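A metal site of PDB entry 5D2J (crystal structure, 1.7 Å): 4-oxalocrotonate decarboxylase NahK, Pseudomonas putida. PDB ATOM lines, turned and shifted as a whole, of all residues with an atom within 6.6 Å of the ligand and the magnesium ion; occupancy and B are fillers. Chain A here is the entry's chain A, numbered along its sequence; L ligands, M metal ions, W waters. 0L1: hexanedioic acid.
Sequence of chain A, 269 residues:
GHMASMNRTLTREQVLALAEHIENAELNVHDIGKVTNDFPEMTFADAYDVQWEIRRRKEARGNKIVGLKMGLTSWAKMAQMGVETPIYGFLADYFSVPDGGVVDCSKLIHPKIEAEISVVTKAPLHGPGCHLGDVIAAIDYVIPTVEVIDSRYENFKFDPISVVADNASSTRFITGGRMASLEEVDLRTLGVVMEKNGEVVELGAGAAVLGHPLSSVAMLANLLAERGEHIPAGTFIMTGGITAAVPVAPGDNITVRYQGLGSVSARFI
The magnesium ion is bound by OE2 of Glu 116 (2.1 Å), OE1 of Glu 147 (2.1 Å), water W2 (2.2 Å), water W1 (2.2 Å), OE1 of Glu 114 (2.2 Å) and O2 of the ligand (2.2 Å).
Within 4 Å of the magnesium ion: Glu 114, Glu 116 and Glu 147. The nearest printed residue that does not touch the magnesium ion is Lys 69 (4.01 Å).
The side-chain hydroxyl (OG) of Ser 169 is in hydrogen-bond range of an oxygen (O4) of the ligand (2.7 Å). An oxygen (O2) of the ligand sits close to the side-chain amino group (NZ) of Lys 69 (3.0 Å). NZ of Lys 77 lies within salt-bridge range of O3 of the ligand, 3.6 Å away.
Gly 71 touches the ligand. Leu 72 touches the ligand. CG2 of Ile 149 touches O2 of the ligand, 3.8 Å away. Ser 151 touches the ligand. Phe 158 touches the ligand. Val 163 touches the ligand. Ala 168 touches the ligand (O to C3, 3.4 Å). The nearest printed residue that does not touch the ligand is Met 70 (4.1 Å).
OE1 of Glu 116 lies within hydrogen-bond range of N of Gly 240 (3.0 Å). OE2 of Glu 147 is in salt-bridge range of NZ of Lys 69 (2.5 Å). The backbone NH of Asp 150 lies within hydrogen-bond range of the backbone carbonyl oxygen of Ser 169 (2.9 Å). NZ of Lys 69 sits at hydrogen-bond distance from O of Ala 168 (3.0 Å). The side-chain amino group of Lys 69 sits close to the side-chain hydroxyl of Ser 170, at 3.3 Å. The backbone NH (N) of Gly 71 sits at hydrogen-bond distance from the backbone carbonyl oxygen (O) of Ile 87. O of Val 163 lies within hydrogen-bond range of N of Ala 168 (2.9 Å). The backbone NH of Ile 149 is in hydrogen-bond range of the backbone carbonyl oxygen of Lys 112, 2.9 Å away.
Water W1 lies within hydrogen-bond range of OE1 of Glu 116 (2.7 Å) and O of Met 70 (2.7 Å). Water W2 lies within hydrogen-bond range of O1 of the ligand (2.6 Å), N of Gly 241 (2.9 Å) and OE2 of Glu 114 (3.0 Å). Water W3 bridges an oxygen (O4) of the ligand and the backbone NH of Ser 151.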
ATOM      1  N   LYS A  69       5.915  15.939 -23.650  1.00  0.00           N
ATOM      2  CA  LYS A  69       5.347  14.927 -24.532  1.00  0.00           C
ATOM      3  C   LYS A  69       4.258  14.144 -23.822  1.00  0.00           C
ATOM      4  O   LYS A  69       4.225  14.090 -22.599  1.00  0.00           O
ATOM      5  CB  LYS A  69       6.419  13.980 -25.096  1.00  0.00           C
ATOM      6  CG  LYS A  69       7.414  13.404 -24.096  1.00  0.00           C
ATOM      7  CD  LYS A  69       6.983  12.044 -23.517  1.00  0.00           C
ATOM      8  CE  LYS A  69       6.700  10.989 -24.595  1.00  0.00           C
ATOM      9  NZ  LYS A  69       7.861  10.094 -24.959  1.00  0.00           N
ATOM     10  N   MET A  70       3.369  13.563 -24.604  1.00  0.00           N
ATOM     11  CA  MET A  70       2.325  12.702 -24.065  1.00  0.00           C
ATOM     12  C   MET A  70       2.550  11.285 -24.569  1.00  0.00           C
ATOM     13  O   MET A  70       2.864  11.083 -25.744  1.00  0.00           O
ATOM     14  CB  MET A  70       0.944  13.212 -24.506  1.00  0.00           C
ATOM     15  CG  MET A  70       0.510  14.451 -23.748  1.00  0.00           C
ATOM     16  SD  MET A  70      -0.081  14.060 -22.086  1.00  0.00           S
ATOM     17  CE  MET A  70      -1.717  13.488 -22.499  1.00  0.00           C
ATOM     18  N   GLY A  71       2.393  10.322 -23.678  1.00  0.00           N
ATOM     19  CA  GLY A  71       2.536   8.923 -24.028  1.00  0.00           C
ATOM     20  C   GLY A  71       1.345   8.080 -23.595  1.00  0.00           C
ATOM     21  O   GLY A  71       0.527   8.536 -22.789  1.00  0.00           O
ATOM     22  N   LEU A  72       1.260   6.871 -24.133  1.00  0.00           N
ATOM     23  CA  LEU A  72       0.114   5.989 -23.886  1.00  0.00           C
ATOM     24  C   LEU A  72      -1.173   6.699 -24.286  1.00  0.00           C
ATOM     25  O   LEU A  72      -2.147   6.739 -23.527  1.00  0.00           O
ATOM     26  CB  LEU A  72       0.061   5.530 -22.422  1.00  0.00           C
ATOM     27  CG  LEU A  72       1.367   4.985 -21.825  1.00  0.00           C
ATOM     28  CD1 LEU A  72       1.115   4.330 -20.467  1.00  0.00           C
ATOM     29  CD2 LEU A  72       2.058   4.012 -22.770  1.00  0.00           C
ATOM     30  N   THR A  73      -1.184   7.261 -25.483  1.00  0.00           N
ATOM     31  CA  THR A  73      -2.320   8.023 -25.961  1.00  0.00           C
ATOM     32  C   THR A  73      -3.264   7.183 -26.834  1.00  0.00           C
ATOM     33  O   THR A  73      -4.127   7.723 -27.513  1.00  0.00           O
ATOM     34  CB  THR A  73      -1.876   9.280 -26.731  1.00  0.00           C
ATOM     35  OG1 THR A  73      -0.965   8.897 -27.782  1.00  0.00           O
ATOM     36  CG2 THR A  73      -1.167  10.263 -25.807  1.00  0.00           C
ATOM     37  N   LYS A  77      -2.939   1.196 -25.917  1.00  0.00           N
ATOM     38  CA  LYS A  77      -1.751   1.457 -25.110  1.00  0.00           C
ATOM     39  C   LYS A  77      -2.053   1.514 -23.622  1.00  0.00           C
ATOM     40  O   LYS A  77      -1.346   0.903 -22.817  1.00  0.00           O
ATOM     41  CB  LYS A  77      -1.080   2.747 -25.578  1.00  0.00           C
ATOM     42  CG  LYS A  77       0.125   2.540 -26.481  1.00  0.00           C
ATOM     43  CD  LYS A  77       1.330   2.065 -25.677  1.00  0.00           C
ATOM     44  CE  LYS A  77       2.618   2.093 -26.491  1.00  0.00           C
ATOM     45  NZ  LYS A  77       3.826   1.807 -25.657  1.00  0.00           N
ATOM     46  N   MET A  81      -0.999  -1.211 -20.392  1.00  0.00           N
ATOM     47  CA  MET A  81      -0.284  -0.711 -19.233  1.00  0.00           C
ATOM     48  C   MET A  81      -1.153  -0.693 -17.971  1.00  0.00           C
ATOM     49  O   MET A  81      -0.692  -0.304 -16.895  1.00  0.00           O
ATOM     50  CB  MET A  81       0.271   0.689 -19.525  1.00  0.00           C
ATOM     51  CG  MET A  81       1.312   0.733 -20.637  1.00  0.00           C
ATOM     52  SD  MET A  81       2.955   0.243 -20.071  1.00  0.00           S
ATOM     53  CE  MET A  81       3.806   0.059 -21.644  1.00  0.00           C
ATOM     54  N   ILE A  87       0.326   9.317 -19.952  1.00  0.00           N
ATOM     55  CA  ILE A  87       1.381   9.829 -19.094  1.00  0.00           C
ATOM     56  C   ILE A  87       2.078  10.930 -19.870  1.00  0.00           C
ATOM     57  O   ILE A  87       1.911  11.065 -21.082  1.00  0.00           O
ATOM     58  CB  ILE A  87       2.398   8.737 -18.713  1.00  0.00           C
ATOM     59  CG1 ILE A  87       3.069   8.158 -19.963  1.00  0.00           C
ATOM     60  CG2 ILE A  87       1.723   7.616 -17.929  1.00  0.00           C
ATOM     61  CD1 ILE A  87       4.209   7.151 -19.654  1.00  0.00           C
ATOM     62  N   LYS A 112      13.494   3.289 -30.962  1.00  0.00           N
ATOM     63  CA  LYS A 112      12.417   3.109 -31.926  1.00  0.00           C
ATOM     64  C   LYS A 112      11.919   4.488 -32.311  1.00  0.00           C
ATOM     65  O   LYS A 112      12.132   5.440 -31.578  1.00  0.00           O
ATOM     66  CB  LYS A 112      11.258   2.331 -31.315  1.00  0.00           C
ATOM     67  CG  LYS A 112      11.537   0.884 -30.981  1.00  0.00           C
ATOM     68  CD  LYS A 112      10.288   0.214 -30.463  1.00  0.00           C
ATOM     69  CE  LYS A 112      10.616  -1.125 -29.814  1.00  0.00           C
ATOM     70  NZ  LYS A 112       9.368  -1.835 -29.427  1.00  0.00           N
ATOM     71  N   GLU A 114       8.458   6.910 -33.712  1.00  0.00           N
ATOM     72  CA  GLU A 114       7.001   7.058 -33.806  1.00  0.00           C
ATOM     73  C   GLU A 114       6.767   8.371 -34.519  1.00  0.00           C
ATOM     74  O   GLU A 114       7.420   9.361 -34.192  1.00  0.00           O
ATOM     75  CB  GLU A 114       6.362   7.267 -32.431  1.00  0.00           C
ATOM     76  CG  GLU A 114       6.605   6.252 -31.349  1.00  0.00           C
ATOM     77  CD  GLU A 114       5.903   6.637 -30.050  1.00  0.00           C
ATOM     78  OE1 GLU A 114       6.349   7.599 -29.366  1.00  0.00           O
ATOM     79  OE2 GLU A 114       4.886   5.998 -29.731  1.00  0.00           O
ATOM     80  N   GLU A 116       4.454  11.664 -34.969  1.00  0.00           N
ATOM     81  CA  GLU A 116       3.508  12.392 -34.135  1.00  0.00           C
ATOM     82  C   GLU A 116       3.240  13.760 -34.753  1.00  0.00           C
ATOM     83  O   GLU A 116       3.894  14.146 -35.723  1.00  0.00           O
ATOM     84  CB  GLU A 116       4.063  12.568 -32.706  1.00  0.00           C
ATOM     85  CG  GLU A 116       4.693  11.293 -32.139  1.00  0.00           C
ATOM     86  CD  GLU A 116       4.803  11.274 -30.627  1.00  0.00           C
ATOM     87  OE1 GLU A 116       4.333  12.219 -29.970  1.00  0.00           O
ATOM     88  OE2 GLU A 116       5.341  10.274 -30.100  1.00  0.00           O
ATOM     89  N   GLU A 147       9.279  11.125 -33.000  1.00  0.00           N
ATOM     90  CA  GLU A 147       9.945  10.892 -31.725  1.00  0.00           C
ATOM     91  C   GLU A 147      10.861   9.698 -31.834  1.00  0.00           C
ATOM     92  O   GLU A 147      10.539   8.721 -32.498  1.00  0.00           O
ATOM     93  CB  GLU A 147       8.971  10.640 -30.563  1.00  0.00           C
ATOM     94  CG  GLU A 147       9.697  10.780 -29.200  1.00  0.00           C
ATOM     95  CD  GLU A 147       8.816  10.620 -27.979  1.00  0.00           C
ATOM     96  OE1 GLU A 147       7.659  10.172 -28.107  1.00  0.00           O
ATOM     97  OE2 GLU A 147       9.310  10.917 -26.866  1.00  0.00           O
ATOM     98  N   ILE A 149      12.018   7.108 -29.243  1.00  0.00           N
ATOM     99  CA  ILE A 149      11.835   6.653 -27.862  1.00  0.00           C
ATOM    100  C   ILE A 149      12.859   5.570 -27.532  1.00  0.00           C
ATOM    101  O   ILE A 149      13.265   4.783 -28.399  1.00  0.00           O
ATOM    102  CB  ILE A 149      10.409   6.135 -27.568  1.00  0.00           C
ATOM    103  CG1 ILE A 149       9.941   5.157 -28.644  1.00  0.00           C
ATOM    104  CG2 ILE A 149       9.440   7.313 -27.426  1.00  0.00           C
ATOM    105  CD1 ILE A 149       8.664   4.415 -28.281  1.00  0.00           C
ATOM    106  N   ASP A 150      13.277   5.514 -26.274  1.00  0.00           N
ATOM    107  CA  ASP A 150      14.376   4.627 -25.933  1.00  0.00           C
ATOM    108  C   ASP A 150      14.357   4.378 -24.442  1.00  0.00           C
ATOM    109  O   ASP A 150      15.086   5.023 -23.691  1.00  0.00           O
ATOM    110  CB  ASP A 150      15.700   5.299 -26.337  1.00  0.00           C
ATOM    111  CG  ASP A 150      16.874   4.353 -26.286  1.00  0.00           C
ATOM    112  OD1 ASP A 150      16.686   3.148 -26.556  1.00  0.00           O
ATOM    113  OD2 ASP A 150      18.001   4.811 -25.968  1.00  0.00           O
ATOM    114  N   SER A 151      13.503   3.457 -24.009  1.00  0.00           N
ATOM    115  CA  SER A 151      13.355   3.164 -22.589  1.00  0.00           C
ATOM    116  C   SER A 151      14.688   2.739 -21.997  1.00  0.00           C
ATOM    117  O   SER A 151      15.421   1.945 -22.584  1.00  0.00           O
ATOM    118  CB  SER A 151      12.335   2.045 -22.379  1.00  0.00           C
ATOM    119  OG  SER A 151      12.282   1.635 -21.017  1.00  0.00           O
ATOM    120  N   PHE A 156      12.667  -3.733 -22.735  1.00  0.00           N
ATOM    121  CA  PHE A 156      11.374  -3.113 -22.539  1.00  0.00           C
ATOM    122  C   PHE A 156      10.577  -3.840 -21.450  1.00  0.00           C
ATOM    123  O   PHE A 156       9.342  -3.828 -21.447  1.00  0.00           O
ATOM    124  CB  PHE A 156      10.631  -3.017 -23.866  1.00  0.00           C
ATOM    125  CG  PHE A 156      11.485  -2.503 -24.990  1.00  0.00           C
ATOM    126  CD1 PHE A 156      11.847  -1.165 -25.062  1.00  0.00           C
ATOM    127  CD2 PHE A 156      11.959  -3.370 -25.976  1.00  0.00           C
ATOM    128  CE1 PHE A 156      12.648  -0.693 -26.084  1.00  0.00           C
ATOM    129  CE2 PHE A 156      12.763  -2.908 -27.002  1.00  0.00           C
ATOM    130  CZ  PHE A 156      13.110  -1.566 -27.065  1.00  0.00           C
ATOM    131  N   PHE A 158       9.202  -3.460 -18.404  1.00  0.00           N
ATOM    132  CA  PHE A 158       8.848  -2.394 -17.473  1.00  0.00           C
ATOM    133  C   PHE A 158       7.375  -2.377 -17.015  1.00  0.00           C
ATOM    134  O   PHE A 158       6.646  -3.352 -17.232  1.00  0.00           O
ATOM    135  CB  PHE A 158       9.239  -1.032 -18.061  1.00  0.00           C
ATOM    136  CG  PHE A 158       8.793  -0.813 -19.482  1.00  0.00           C
ATOM    137  CD1 PHE A 158       7.481  -1.023 -19.868  1.00  0.00           C
ATOM    138  CD2 PHE A 158       9.697  -0.350 -20.431  1.00  0.00           C
ATOM    139  CE1 PHE A 158       7.076  -0.802 -21.172  1.00  0.00           C
ATOM    140  CE2 PHE A 158       9.304  -0.124 -21.739  1.00  0.00           C
ATOM    141  CZ  PHE A 158       7.989  -0.351 -22.112  1.00  0.00           C
ATOM    142  N   VAL A 163       8.086   3.585 -16.092  1.00  0.00           N
ATOM    143  CA  VAL A 163       8.202   4.373 -17.317  1.00  0.00           C
ATOM    144  C   VAL A 163       8.063   5.869 -17.046  1.00  0.00           C
ATOM    145  O   VAL A 163       8.822   6.676 -17.607  1.00  0.00           O
ATOM    146  CB  VAL A 163       7.186   3.892 -18.377  1.00  0.00           C
ATOM    147  CG1 VAL A 163       7.089   4.871 -19.545  1.00  0.00           C
ATOM    148  CG2 VAL A 163       7.601   2.509 -18.853  1.00  0.00           C
ATOM    149  N   ASN A 167      10.994   9.266 -17.435  1.00  0.00           N
ATOM    150  CA  ASN A 167      10.611  10.368 -18.326  1.00  0.00           C
ATOM    151  C   ASN A 167       9.915   9.883 -19.599  1.00  0.00           C
ATOM    152  O   ASN A 167      10.129  10.433 -20.674  1.00  0.00           O
ATOM    153  CB  ASN A 167      11.821  11.243 -18.681  1.00  0.00           C
ATOM    154  CG  ASN A 167      11.413  12.562 -19.308  1.00  0.00           C
ATOM    155  OD1 ASN A 167      10.353  13.103 -18.984  1.00  0.00           O
ATOM    156  ND2 ASN A 167      12.252  13.094 -20.199  1.00  0.00           N
ATOM    157  N   ALA A 168       9.113   8.842 -19.456  1.00  0.00           N
ATOM    158  CA  ALA A 168       8.330   8.290 -20.558  1.00  0.00           C
ATOM    159  C   ALA A 168       9.198   7.929 -21.761  1.00  0.00           C
ATOM    160  O   ALA A 168       8.779   8.118 -22.901  1.00  0.00           O
ATOM    161  CB  ALA A 168       7.239   9.278 -20.987  1.00  0.00           C
ATOM    162  N   SER A 169      10.410   7.427 -21.505  1.00  0.00           N
ATOM    163  CA  SER A 169      11.299   6.920 -22.564  1.00  0.00           C
ATOM    164  C   SER A 169      11.804   7.978 -23.555  1.00  0.00           C
ATOM    165  O   SER A 169      12.325   7.630 -24.619  1.00  0.00           O
ATOM    166  CB  SER A 169      10.615   5.794 -23.351  1.00  0.00           C
ATOM    167  OG  SER A 169      10.165   4.753 -22.483  1.00  0.00           O
ATOM    168  N   SER A 170      11.658   9.255 -23.205  1.00  0.00           N
ATOM    169  CA  SER A 170      12.096  10.329 -24.084  1.00  0.00           C
ATOM    170  C   SER A 170      13.607  10.352 -24.318  1.00  0.00           C
ATOM    171  O   SER A 170      14.386  10.105 -23.392  1.00  0.00           O
ATOM    172  CB  SER A 170      11.664  11.687 -23.522  1.00  0.00           C
ATOM    173  OG  SER A 170      10.274  11.684 -23.276  1.00  0.00           O
ATOM    174  N   MET A 238       4.479  17.467 -27.835  1.00  0.00           N
ATOM    175  CA  MET A 238       4.371  16.309 -28.735  1.00  0.00           C
ATOM    176  C   MET A 238       3.182  15.481 -28.282  1.00  0.00           C
ATOM    177  O   MET A 238       3.205  14.897 -27.195  1.00  0.00           O
ATOM    178  CB  MET A 238       5.650  15.474 -28.692  1.00  0.00           C
ATOM    179  CG  MET A 238       6.842  16.186 -29.277  1.00  0.00           C
ATOM    180  SD  MET A 238       8.257  15.088 -29.371  1.00  0.00           S
ATOM    181  CE  MET A 238       7.497  13.724 -30.234  1.00  0.00           C
ATOM    182  N   THR A 239       2.142  15.426 -29.108  1.00  0.00           N
ATOM    183  CA  THR A 239       0.848  14.961 -28.612  1.00  0.00           C
ATOM    184  C   THR A 239       0.615  13.469 -28.503  1.00  0.00           C
ATOM    185  O   THR A 239      -0.336  13.045 -27.847  1.00  0.00           O
ATOM    186  CB  THR A 239      -0.339  15.609 -29.364  1.00  0.00           C
ATOM    187  OG1 THR A 239      -0.277  15.271 -30.759  1.00  0.00           O
ATOM    188  CG2 THR A 239      -0.286  17.140 -29.213  1.00  0.00           C
ATOM    189  N   GLY A 240       1.475  12.662 -29.136  1.00  0.00           N
ATOM    190  CA  GLY A 240       1.355  11.215 -29.029  1.00  0.00           C
ATOM    191  C   GLY A 240       1.596  10.450 -30.325  1.00  0.00           C
ATOM    192  O   GLY A 240       1.521  11.019 -31.412  1.00  0.00           O
ATOM    193  N   GLY A 241       1.857   9.154 -30.203  1.00  0.00           N
ATOM    194  CA  GLY A 241       2.146   8.334 -31.373  1.00  0.00           C
ATOM    195  C   GLY A 241       0.962   8.156 -32.311  1.00  0.00           C
ATOM    196  O   GLY A 241      -0.091   7.634 -31.915  1.00  0.00           O
ATOM    197  N   ALA A 245       5.411   2.168 -33.098  1.00  0.00           N
ATOM    198  CA  ALA A 245       6.844   2.416 -32.989  1.00  0.00           C
ATOM    199  C   ALA A 245       7.662   1.381 -33.786  1.00  0.00           C
ATOM    200  O   ALA A 245       7.323   0.208 -33.814  1.00  0.00           O
ATOM    201  CB  ALA A 245       7.264   2.433 -31.537  1.00  0.00           C
HETATM  202  O1  0L1 L   1       4.269   6.971 -26.042  1.00  0.00           O
HETATM  203  C2  0L1 L   1       5.374   7.435 -25.671  1.00  0.00           C
HETATM  204  O2  0L1 L   1       5.918   8.352 -26.338  1.00  0.00           O
HETATM  205  C3  0L1 L   1       6.056   6.898 -24.428  1.00  0.00           C
HETATM  206  C4  0L1 L   1       6.164   5.385 -24.498  1.00  0.00           C
HETATM  207  C5  0L1 L   1       6.934   4.881 -23.304  1.00  0.00           C
HETATM  208  C6  0L1 L   1       6.940   3.368 -23.246  1.00  0.00           C
HETATM  209  C7  0L1 L   1       7.877   2.777 -24.282  1.00  0.00           C
HETATM  210  O4  0L1 L   1       9.114   3.020 -24.224  1.00  0.00           O
HETATM  211  O3  0L1 L   1       7.433   2.025 -25.200  1.00  0.00           O
HETATM  212 MG    MG M   1       5.716   9.375 -28.273  1.00  0.00          MG
HETATM  213  O   HOH W   1       4.871  11.232 -27.538  1.00  0.00           O
HETATM  214  O   HOH W   2       3.845   8.300 -28.201  1.00  0.00           O
HETATM  215  O   HOH W   3      11.144   2.163 -25.641  1.00  0.00           O
HETATM  216  O   HOH W   4       9.269   0.107 -26.389  1.00  0.00           O
